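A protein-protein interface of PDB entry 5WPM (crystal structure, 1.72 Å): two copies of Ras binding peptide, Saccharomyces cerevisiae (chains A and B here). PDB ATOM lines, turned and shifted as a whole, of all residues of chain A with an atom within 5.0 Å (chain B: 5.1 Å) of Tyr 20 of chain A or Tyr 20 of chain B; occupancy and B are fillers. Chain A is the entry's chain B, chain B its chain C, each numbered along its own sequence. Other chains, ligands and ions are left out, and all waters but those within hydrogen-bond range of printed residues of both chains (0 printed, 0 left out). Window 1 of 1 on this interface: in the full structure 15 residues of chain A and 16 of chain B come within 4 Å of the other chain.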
ATOM      1  N   PRO A   5       2.777 -32.003   4.573  1.00  0.00           N
ATOM      2  CA  PRO A   5       3.215 -32.144   5.961  1.00  0.00           C
ATOM      3  C   PRO A   5       3.030 -30.826   6.709  1.00  0.00           C
ATOM      4  O   PRO A   5       3.118 -29.766   6.097  1.00  0.00           O
ATOM      5  CB  PRO A   5       4.692 -32.512   5.829  1.00  0.00           C
ATOM      6  CG  PRO A   5       5.123 -31.927   4.531  1.00  0.00           C
ATOM      7  CD  PRO A   5       3.913 -31.855   3.642  1.00  0.00           C
ATOM      8  N   ARG A   6       2.729 -30.898   8.002  1.00  0.00           N
ATOM      9  CA  ARG A   6       2.681 -29.703   8.856  1.00  0.00           C
ATOM     10  C   ARG A   6       4.053 -29.453   9.469  1.00  0.00           C
ATOM     11  O   ARG A   6       4.736 -30.406   9.855  1.00  0.00           O
ATOM     12  CB  ARG A   6       1.656 -29.875   9.973  1.00  0.00           C
ATOM     13  CG  ARG A   6       0.247 -30.138   9.474  1.00  0.00           C
ATOM     14  CD  ARG A   6      -0.777 -29.951  10.574  1.00  0.00           C
ATOM     15  NE  ARG A   6      -2.139 -30.181  10.082  1.00  0.00           N
ATOM     16  CZ  ARG A   6      -3.021 -29.241   9.722  1.00  0.00           C
ATOM     17  NH1 ARG A   6      -2.739 -27.939   9.777  1.00  0.00           N
ATOM     18  NH2 ARG A   6      -4.224 -29.614   9.297  1.00  0.00           N
ATOM     19  N   CYS A   7       4.453 -28.186   9.566  1.00  0.00           N
ATOM     20  CA  CYS A   7       5.694 -27.820  10.273  1.00  0.00           C
ATOM     21  C   CYS A   7       5.542 -28.235  11.734  1.00  0.00           C
ATOM     22  O   CYS A   7       4.490 -27.978  12.322  1.00  0.00           O
ATOM     23  CB  CYS A   7       5.969 -26.317  10.186  1.00  0.00           C
ATOM     24  SG  CYS A   7       7.591 -25.788  10.816  1.00  0.00           S
ATOM     25  N   PRO A   8       6.575 -28.876  12.330  1.00  0.00           N
ATOM     26  CA  PRO A   8       6.391 -29.396  13.691  1.00  0.00           C
ATOM     27  C   PRO A   8       6.576 -28.366  14.824  1.00  0.00           C
ATOM     28  O   PRO A   8       6.598 -28.762  15.989  1.00  0.00           O
ATOM     29  CB  PRO A   8       7.439 -30.517  13.774  1.00  0.00           C
ATOM     30  CG  PRO A   8       8.494 -30.149  12.783  1.00  0.00           C
ATOM     31  CD  PRO A   8       7.964 -29.080  11.870  1.00  0.00           C
ATOM     32  N   ASP A  16      13.598 -33.351  14.251  1.00  0.00           N
ATOM     33  CA  ASP A  16      12.222 -33.193  13.769  1.00  0.00           C
ATOM     34  C   ASP A  16      12.160 -32.348  12.492  1.00  0.00           C
ATOM     35  O   ASP A  16      11.402 -32.659  11.585  1.00  0.00           O
ATOM     36  CB  ASP A  16      11.323 -32.600  14.854  1.00  0.00           C
ATOM     37  CG  ASP A  16      11.162 -33.526  16.052  1.00  0.00           C
ATOM     38  OD1 ASP A  16      10.680 -34.663  15.885  1.00  0.00           O
ATOM     39  OD2 ASP A  16      11.534 -33.120  17.168  1.00  0.00           O
ATOM     40  N   LEU A  17      12.977 -31.299  12.419  1.00  0.00           N
ATOM     41  CA  LEU A  17      13.070 -30.483  11.204  1.00  0.00           C
ATOM     42  C   LEU A  17      13.615 -31.262  10.006  1.00  0.00           C
ATOM     43  O   LEU A  17      13.147 -31.070   8.881  1.00  0.00           O
ATOM     44  CB  LEU A  17      13.926 -29.234  11.448  1.00  0.00           C
ATOM     45  CG  LEU A  17      13.265 -28.165  12.324  1.00  0.00           C
ATOM     46  CD1 LEU A  17      14.292 -27.110  12.708  1.00  0.00           C
ATOM     47  CD2 LEU A  17      12.076 -27.509  11.641  1.00  0.00           C
ATOM     48  N   HIS A  18      14.600 -32.127  10.250  1.00  0.00           N
ATOM     49  CA  HIS A  18      15.135 -33.002   9.203  1.00  0.00           C
ATOM     50  C   HIS A  18      14.067 -33.967   8.693  1.00  0.00           C
ATOM     51  O   HIS A  18      13.931 -34.167   7.493  1.00  0.00           O
ATOM     52  CB  HIS A  18      16.336 -33.813   9.689  1.00  0.00           C
ATOM     53  CG  HIS A  18      17.649 -33.111   9.543  1.00  0.00           C
ATOM     54  ND1 HIS A  18      18.256 -32.920   8.321  1.00  0.00           N
ATOM     55  CD2 HIS A  18      18.481 -32.570  10.467  1.00  0.00           C
ATOM     56  CE1 HIS A  18      19.401 -32.281   8.497  1.00  0.00           C
ATOM     57  NE2 HIS A  18      19.561 -32.061   9.790  1.00  0.00           N
ATOM     58  N   GLU A  19      13.326 -34.566   9.616  1.00  0.00           N
ATOM     59  CA  GLU A  19      12.206 -35.454   9.250  1.00  0.00           C
ATOM     60  C   GLU A  19      11.153 -34.720   8.414  1.00  0.00           C
ATOM     61  O   GLU A  19      10.657 -35.242   7.400  1.00  0.00           O
ATOM     62  CB  GLU A  19      11.585 -36.054  10.510  1.00  0.00           C
ATOM     63  CG  GLU A  19      12.427 -37.148  11.155  1.00  0.00           C
ATOM     64  CD  GLU A  19      12.415 -38.470  10.393  1.00  0.00           C
ATOM     65  OE1 GLU A  19      11.458 -38.741   9.632  1.00  0.00           O
ATOM     66  OE2 GLU A  19      13.380 -39.246  10.559  1.00  0.00           O
ATOM     67  N   TYR A  20      10.838 -33.500   8.835  1.00  0.00           N
ATOM     68  CA  TYR A  20       9.916 -32.636   8.104  1.00  0.00           C
ATOM     69  C   TYR A  20      10.456 -32.230   6.727  1.00  0.00           C
ATOM     70  O   TYR A  20       9.705 -32.206   5.745  1.00  0.00           O
ATOM     71  CB  TYR A  20       9.585 -31.401   8.941  1.00  0.00           C
ATOM     72  CG  TYR A  20       8.821 -30.354   8.193  1.00  0.00           C
ATOM     73  CD1 TYR A  20       7.451 -30.471   7.975  1.00  0.00           C
ATOM     74  CD2 TYR A  20       9.464 -29.265   7.675  1.00  0.00           C
ATOM     75  CE1 TYR A  20       6.749 -29.500   7.274  1.00  0.00           C
ATOM     76  CE2 TYR A  20       8.779 -28.304   6.976  1.00  0.00           C
ATOM     77  CZ  TYR A  20       7.418 -28.415   6.774  1.00  0.00           C
ATOM     78  OH  TYR A  20       6.763 -27.427   6.074  1.00  0.00           O
ATOM     79  N   TRP A  21      11.747 -31.906   6.665  1.00  0.00           N
ATOM     80  CA  TRP A  21      12.383 -31.537   5.406  1.00  0.00           C
ATOM     81  C   TRP A  21      12.273 -32.652   4.363  1.00  0.00           C
ATOM     82  O   TRP A  21      11.982 -32.373   3.198  1.00  0.00           O
ATOM     83  CB  TRP A  21      13.862 -31.164   5.590  1.00  0.00           C
ATOM     84  CG  TRP A  21      14.468 -30.698   4.306  1.00  0.00           C
ATOM     85  CD1 TRP A  21      14.476 -29.425   3.817  1.00  0.00           C
ATOM     86  CD2 TRP A  21      15.110 -31.512   3.316  1.00  0.00           C
ATOM     87  NE1 TRP A  21      15.098 -29.394   2.595  1.00  0.00           N
ATOM     88  CE2 TRP A  21      15.494 -30.661   2.262  1.00  0.00           C
ATOM     89  CE3 TRP A  21      15.409 -32.877   3.226  1.00  0.00           C
ATOM     90  CZ2 TRP A  21      16.157 -31.131   1.117  1.00  0.00           C
ATOM     91  CZ3 TRP A  21      16.067 -33.347   2.086  1.00  0.00           C
ATOM     92  CH2 TRP A  21      16.439 -32.468   1.053  1.00  0.00           C
ATOM     93  N   ALA A  22      12.519 -33.892   4.783  1.00  0.00           N
ATOM     94  CA  ALA A  22      12.451 -35.043   3.871  1.00  0.00           C
ATOM     95  C   ALA A  22      11.016 -35.287   3.401  1.00  0.00           C
ATOM     96  O   ALA A  22      10.803 -35.640   2.244  1.00  0.00           O
ATOM     97  CB  ALA A  22      13.015 -36.289   4.520  1.00  0.00           C
ATOM     98  N   ARG A  23      10.041 -35.092   4.283  1.00  0.00           N
ATOM     99  CA  ARG A  23       8.623 -35.180   3.865  1.00  0.00           C
ATOM    100  C   ARG A  23       8.257 -34.085   2.851  1.00  0.00           C
ATOM    101  O   ARG A  23       7.582 -34.356   1.845  1.00  0.00           O
ATOM    102  CB  ARG A  23       7.685 -35.135   5.076  1.00  0.00           C
ATOM    103  CG  ARG A  23       7.754 -36.373   5.956  1.00  0.00           C
ATOM    104  CD  ARG A  23       6.958 -36.177   7.237  1.00  0.00           C
ATOM    105  NE  ARG A  23       6.843 -37.413   8.018  1.00  0.00           N
ATOM    106  CZ  ARG A  23       7.447 -37.687   9.182  1.00  0.00           C
ATOM    107  NH1 ARG A  23       8.249 -36.813   9.790  1.00  0.00           N
ATOM    108  NH2 ARG A  23       7.235 -38.868   9.762  1.00  0.00           N
ATOM    109  N   LEU A  24       8.694 -32.853   3.118  1.00  0.00           N
ATOM    110  CA  LEU A  24       8.460 -31.722   2.201  1.00  0.00           C
ATOM    111  C   LEU A  24       9.073 -31.950   0.825  1.00  0.00           C
ATOM    112  O   LEU A  24       8.453 -31.638  -0.200  1.00  0.00           O
ATOM    113  CB  LEU A  24       9.017 -30.407   2.769  1.00  0.00           C
ATOM    114  CG  LEU A  24       8.106 -29.391   3.451  1.00  0.00           C
ATOM    115  CD1 LEU A  24       8.938 -28.130   3.704  1.00  0.00           C
ATOM    116  CD2 LEU A  24       6.861 -29.045   2.641  1.00  0.00           C
ATOM    117  N   TRP A  25      10.292 -32.481   0.818  1.00  0.00           N
ATOM    118  CA  TRP A  25      11.013 -32.791  -0.415  1.00  0.00           C
ATOM    119  C   TRP A  25      10.139 -33.646  -1.326  1.00  0.00           C
ATOM    120  O   TRP A  25       9.939 -33.311  -2.491  1.00  0.00           O
ATOM    121  CB  TRP A  25      12.319 -33.519  -0.092  1.00  0.00           C
ATOM    122  CG  TRP A  25      13.279 -33.682  -1.240  1.00  0.00           C
ATOM    123  CD1 TRP A  25      13.323 -32.956  -2.400  1.00  0.00           C
ATOM    124  CD2 TRP A  25      14.375 -34.597  -1.301  1.00  0.00           C
ATOM    125  NE1 TRP A  25      14.359 -33.389  -3.191  1.00  0.00           N
ATOM    126  CE2 TRP A  25      15.028 -34.388  -2.538  1.00  0.00           C
ATOM    127  CE3 TRP A  25      14.873 -35.573  -0.428  1.00  0.00           C
ATOM    128  CZ2 TRP A  25      16.149 -35.132  -2.929  1.00  0.00           C
ATOM    129  CZ3 TRP A  25      15.983 -36.313  -0.816  1.00  0.00           C
ATOM    130  CH2 TRP A  25      16.607 -36.088  -2.058  1.00  0.00           C
ATOM    131  N   PRO B   5      14.707 -20.347   9.711  1.00  0.00           N
ATOM    132  CA  PRO B   5      13.486 -19.859   9.065  1.00  0.00           C
ATOM    133  C   PRO B   5      12.266 -20.280   9.880  1.00  0.00           C
ATOM    134  O   PRO B   5      12.269 -21.373  10.448  1.00  0.00           O
ATOM    135  CB  PRO B   5      13.514 -20.549   7.697  1.00  0.00           C
ATOM    136  CG  PRO B   5      14.307 -21.781   7.910  1.00  0.00           C
ATOM    137  CD  PRO B   5      15.343 -21.435   8.945  1.00  0.00           C
ATOM    138  N   ARG B   6      11.261 -19.409   9.981  1.00  0.00           N
ATOM    139  CA  ARG B   6      10.047 -19.731  10.754  1.00  0.00           C
ATOM    140  C   ARG B   6       9.171 -20.687   9.973  1.00  0.00           C
ATOM    141  O   ARG B   6       9.234 -20.730   8.737  1.00  0.00           O
ATOM    142  CB  ARG B   6       9.247 -18.479  11.137  1.00  0.00           C
ATOM    143  CG  ARG B   6       9.747 -17.817  12.418  1.00  0.00           C
ATOM    144  CD  ARG B   6       9.259 -16.384  12.563  1.00  0.00           C
ATOM    145  NE  ARG B   6       9.899 -15.491  11.593  1.00  0.00           N
ATOM    146  CZ  ARG B   6       9.776 -14.162  11.566  1.00  0.00           C
ATOM    147  NH1 ARG B   6       9.031 -13.515  12.461  1.00  0.00           N
ATOM    148  NH2 ARG B   6      10.412 -13.466  10.626  1.00  0.00           N
ATOM    149  N   CYS B   7       8.357 -21.451  10.702  1.00  0.00           N
ATOM    150  CA  CYS B   7       7.375 -22.338  10.080  1.00  0.00           C
ATOM    151  C   CYS B   7       6.581 -21.535   9.032  1.00  0.00           C
ATOM    152  O   CYS B   7       6.151 -20.417   9.302  1.00  0.00           O
ATOM    153  CB  CYS B   7       6.438 -22.968  11.126  1.00  0.00           C
ATOM    154  SG  CYS B   7       7.158 -24.296  12.142  1.00  0.00           S
ATOM    155  N   PRO B   8       6.415 -22.088   7.823  1.00  0.00           N
ATOM    156  CA  PRO B   8       5.842 -21.336   6.697  1.00  0.00           C
ATOM    157  C   PRO B   8       4.352 -20.967   6.848  1.00  0.00           C
ATOM    158  O   PRO B   8       3.879 -20.032   6.197  1.00  0.00           O
ATOM    159  CB  PRO B   8       6.039 -22.295   5.520  1.00  0.00           C
ATOM    160  CG  PRO B   8       5.981 -23.650   6.148  1.00  0.00           C
ATOM    161  CD  PRO B   8       6.653 -23.500   7.474  1.00  0.00           C
ATOM    162  N   ASP B  16       6.018 -20.357  -1.822  1.00  0.00           N
ATOM    163  CA  ASP B  16       6.514 -20.025  -0.477  1.00  0.00           C
ATOM    164  C   ASP B  16       7.035 -21.251   0.279  1.00  0.00           C
ATOM    165  O   ASP B  16       8.028 -21.147   1.004  1.00  0.00           O
ATOM    166  CB  ASP B  16       5.445 -19.284   0.339  1.00  0.00           C
ATOM    167  CG  ASP B  16       5.274 -17.828  -0.093  1.00  0.00           C
ATOM    168  OD1 ASP B  16       5.797 -17.442  -1.160  1.00  0.00           O
ATOM    169  OD2 ASP B  16       4.621 -17.058   0.642  1.00  0.00           O
ATOM    170  N   LEU B  17       6.391 -22.407   0.099  1.00  0.00           N
ATOM    171  CA  LEU B  17       6.879 -23.655   0.715  1.00  0.00           C
ATOM    172  C   LEU B  17       8.197 -24.119   0.105  1.00  0.00           C
ATOM    173  O   LEU B  17       9.064 -24.640   0.822  1.00  0.00           O
ATOM    174  CB  LEU B  17       5.849 -24.796   0.638  1.00  0.00           C
ATOM    175  CG  LEU B  17       4.815 -24.942   1.754  1.00  0.00           C
ATOM    176  CD1 LEU B  17       3.978 -26.184   1.492  1.00  0.00           C
ATOM    177  CD2 LEU B  17       5.450 -25.033   3.135  1.00  0.00           C
ATOM    178  N   HIS B  18       8.330 -23.945  -1.212  1.00  0.00           N
ATOM    179  CA  HIS B  18       9.589 -24.204  -1.922  1.00  0.00           C
ATOM    180  C   HIS B  18      10.714 -23.330  -1.350  1.00  0.00           C
ATOM    181  O   HIS B  18      11.796 -23.837  -1.043  1.00  0.00           O
ATOM    182  CB  HIS B  18       9.425 -23.947  -3.428  1.00  0.00           C
ATOM    183  CG  HIS B  18      10.488 -24.571  -4.282  1.00  0.00           C
ATOM    184  ND1 HIS B  18      10.248 -24.991  -5.573  1.00  0.00           N
ATOM    185  CD2 HIS B  18      11.792 -24.845  -4.039  1.00  0.00           C
ATOM    186  CE1 HIS B  18      11.358 -25.490  -6.087  1.00  0.00           C
ATOM    187  NE2 HIS B  18      12.309 -25.415  -5.175  1.00  0.00           N
ATOM    188  N   GLU B  19      10.455 -22.030  -1.204  1.00  0.00           N
ATOM    189  CA  GLU B  19      11.428 -21.101  -0.602  1.00  0.00           C
ATOM    190  C   GLU B  19      11.818 -21.581   0.794  1.00  0.00           C
ATOM    191  O   GLU B  19      13.001 -21.695   1.109  1.00  0.00           O
ATOM    192  CB  GLU B  19      10.877 -19.662  -0.546  1.00  0.00           C
ATOM    193  CG  GLU B  19      11.786 -18.656   0.170  1.00  0.00           C
ATOM    194  CD  GLU B  19      11.341 -17.206   0.046  1.00  0.00           C
ATOM    195  OE1 GLU B  19      10.161 -16.944  -0.279  1.00  0.00           O
ATOM    196  OE2 GLU B  19      12.182 -16.313   0.294  1.00  0.00           O
ATOM    197  N   TYR B  20      10.817 -21.874   1.619  1.00  0.00           N
ATOM    198  CA  TYR B  20      11.068 -22.364   2.977  1.00  0.00           C
ATOM    199  C   TYR B  20      11.873 -23.677   2.996  1.00  0.00           C
ATOM    200  O   TYR B  20      12.806 -23.820   3.779  1.00  0.00           O
ATOM    201  CB  TYR B  20       9.752 -22.498   3.761  1.00  0.00           C
ATOM    202  CG  TYR B  20       9.924 -23.189   5.089  1.00  0.00           C
ATOM    203  CD1 TYR B  20      10.576 -22.562   6.153  1.00  0.00           C
ATOM    204  CD2 TYR B  20       9.467 -24.475   5.278  1.00  0.00           C
ATOM    205  CE1 TYR B  20      10.751 -23.205   7.367  1.00  0.00           C
ATOM    206  CE2 TYR B  20       9.638 -25.115   6.478  1.00  0.00           C
ATOM    207  CZ  TYR B  20      10.281 -24.489   7.524  1.00  0.00           C
ATOM    208  OH  TYR B  20      10.425 -25.174   8.703  1.00  0.00           O
ATOM    209  N   TRP B  21      11.513 -24.622   2.128  1.00  0.00           N
ATOM    210  CA  TRP B  21      12.234 -25.893   1.986  1.00  0.00           C
ATOM    211  C   TRP B  21      13.729 -25.690   1.706  1.00  0.00           C
ATOM    212  O   TRP B  21      14.577 -26.292   2.371  1.00  0.00           O
ATOM    213  CB  TRP B  21      11.576 -26.736   0.883  1.00  0.00           C
ATOM    214  CG  TRP B  21      12.349 -27.917   0.366  1.00  0.00           C
ATOM    215  CD1 TRP B  21      12.371 -29.182   0.877  1.00  0.00           C
ATOM    216  CD2 TRP B  21      13.157 -27.948  -0.810  1.00  0.00           C
ATOM    217  NE1 TRP B  21      13.159 -29.992   0.099  1.00  0.00           N
ATOM    218  CE2 TRP B  21      13.659 -29.258  -0.941  1.00  0.00           C
ATOM    219  CE3 TRP B  21      13.515 -26.988  -1.761  1.00  0.00           C
ATOM    220  CZ2 TRP B  21      14.503 -29.631  -1.990  1.00  0.00           C
ATOM    221  CZ3 TRP B  21      14.349 -27.355  -2.795  1.00  0.00           C
ATOM    222  CH2 TRP B  21      14.835 -28.662  -2.901  1.00  0.00           C
ATOM    223  N   ALA B  22      14.037 -24.825   0.744  1.00  0.00           N
ATOM    224  CA  ALA B  22      15.432 -24.510   0.400  1.00  0.00           C
ATOM    225  C   ALA B  22      16.156 -23.853   1.568  1.00  0.00           C
ATOM    226  O   ALA B  22      17.289 -24.219   1.888  1.00  0.00           O
ATOM    227  CB  ALA B  22      15.491 -23.599  -0.810  1.00  0.00           C
ATOM    228  N   ARG B  23      15.499 -22.881   2.189  1.00  0.00           N
ATOM    229  CA  ARG B  23      16.102 -22.149   3.306  1.00  0.00           C
ATOM    230  C   ARG B  23      16.287 -23.026   4.537  1.00  0.00           C
ATOM    231  O   ARG B  23      17.275 -22.883   5.266  1.00  0.00           O
ATOM    232  CB  ARG B  23      15.284 -20.912   3.641  1.00  0.00           C
ATOM    233  CG  ARG B  23      15.414 -19.825   2.586  1.00  0.00           C
ATOM    234  CD  ARG B  23      14.225 -18.901   2.641  1.00  0.00           C
ATOM    235  NE  ARG B  23      14.082 -18.366   3.991  1.00  0.00           N
ATOM    236  CZ  ARG B  23      12.937 -18.220   4.662  1.00  0.00           C
ATOM    237  NH1 ARG B  23      11.750 -18.553   4.143  1.00  0.00           N
ATOM    238  NH2 ARG B  23      12.986 -17.728   5.890  1.00  0.00           N
ATOM    239  N   LEU B  24      15.352 -23.944   4.760  1.00  0.00           N
ATOM    240  CA  LEU B  24      15.486 -24.906   5.848  1.00  0.00           C
ATOM    241  C   LEU B  24      16.707 -25.798   5.622  1.00  0.00           C
ATOM    242  O   LEU B  24      17.500 -25.989   6.545  1.00  0.00           O
ATOM    243  CB  LEU B  24      14.203 -25.736   6.019  1.00  0.00           C
ATOM    244  CG  LEU B  24      14.187 -26.821   7.102  1.00  0.00           C
ATOM    245  CD1 LEU B  24      14.474 -26.263   8.495  1.00  0.00           C
ATOM    246  CD2 LEU B  24      12.834 -27.528   7.071  1.00  0.00           C
ATOM    247  N   TRP B  25      16.895 -26.313   4.402  1.00  0.00           N
ATOM    248  CA  TRP B  25      18.088 -27.117   4.150  1.00  0.00           C
ATOM    249  C   TRP B  25      19.378 -26.340   4.457  1.00  0.00           C
ATOM    250  O   TRP B  25      20.265 -26.855   5.144  1.00  0.00           O
ATOM    251  CB  TRP B  25      18.174 -27.670   2.732  1.00  0.00           C
ATOM    252  CG  TRP B  25      19.346 -28.576   2.665  1.00  0.00           C
ATOM    253  CD1 TRP B  25      20.559 -28.315   2.094  1.00  0.00           C
ATOM    254  CD2 TRP B  25      19.465 -29.850   3.303  1.00  0.00           C
ATOM    255  NE1 TRP B  25      21.410 -29.369   2.300  1.00  0.00           N
ATOM    256  CE2 TRP B  25      20.766 -30.327   3.040  1.00  0.00           C
ATOM    257  CE3 TRP B  25      18.592 -30.643   4.065  1.00  0.00           C
ATOM    258  CZ2 TRP B  25      21.219 -31.573   3.501  1.00  0.00           C
ATOM    259  CZ3 TRP B  25      19.038 -31.885   4.522  1.00  0.00           C
ATOM    260  CH2 TRP B  25      20.343 -32.336   4.240  1.00  0.00           C
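The side-chain sulfur of Cys 7 of chain A sits at hydrogen-bond distance from the side-chain hydroxyl of Tyr 20 of chain B (3.6 Å).
SG of Cys 7 of chain A forms a disulfide with SG of Cys 7 of chain B.
The backbone carbonyl oxygen of Trp 21 of chain B sits at hydrogen-bond distance from the indole nitrogen of Trp 21 of chain A (3.2 Å).
Among the printed residues, merely in contact across the chains: Tyr 20 of chain A with Tyr 20 of chain B (3.3 Å), Trp 21 of chain A with Trp 25 of chain B (3.5 Å), Trp 25 of chain A with Trp 21 of chain B (3.6 Å), Tyr 20 of chain A with Leu 24 of chain B (3.8 Å), Tyr 20 of chain A with Pro 8 of chain B (3.9 Å), Cys 7 of chain A with Pro 8 of chain B (3.97 Å) and Leu 17 of chain A with Leu 24 of chain B (3.99 Å).
Pro 5 of chain A touches none of the printed residues of chain B.
Of the printed residues of chain B, Leu 17 of chain A touches Leu 24 (3.99 Å).
Printed residues of chain B within 4 Å of Trp 25 of chain A: Trp 21 (3.6 Å).
Of the printed residues of chain A, Pro 8 of chain B touches Cys 7 and Tyr 20.
Printed residues of chain A within 4 Å of Tyr 20 of chain B: Cys 7 (3.6 Å) and Tyr 20 (3.3 Å).
Of the printed residues of chain A, Trp 25 of chain B touches Trp 21.
The nearest printed residue of chain A that does not touch Tyr 20 of chain B is Leu 24 of chain A (4.01 Å).
The nearest printed residue of chain A that does not touch Cys 7 of chain B is Pro 8 of chain A (4.6 Å).
Of the 14 printed residues of chain A, 5 touch a printed residue of chain B.
Hydrophobic or aromatic side chains of chain A within 4 Å of the printed part of chain B: Tyr 20, Trp 21 and Trp 25.
Hydrophobic or aromatic side chains of chain B that line the printed part of chain A: Pro 8, Tyr 20, Trp 21, Leu 24 and Trp 25.
Cys 7 of chain A touches its own counterpart, Cys 7 of chain B.
Leu 17 of chain A touches Leu 24 of chain B, but with the chains exchanged Leu 24 of chain A does not touch Leu 17 of chain B (4.2 Å).
Tyr 20 of chain A touches its own counterpart, Tyr 20 of chain B.
Tyr 20 of chain A touches Leu 24 of chain B, but with the chains exchanged Leu 24 of chain A does not touch Tyr 20 of chain B (4.01 Å).
14 positions are printed for both chains.
Of the 10 pairs that touch across the chains among the printed residues, 5 have their exchanged pair printed and touching as well.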
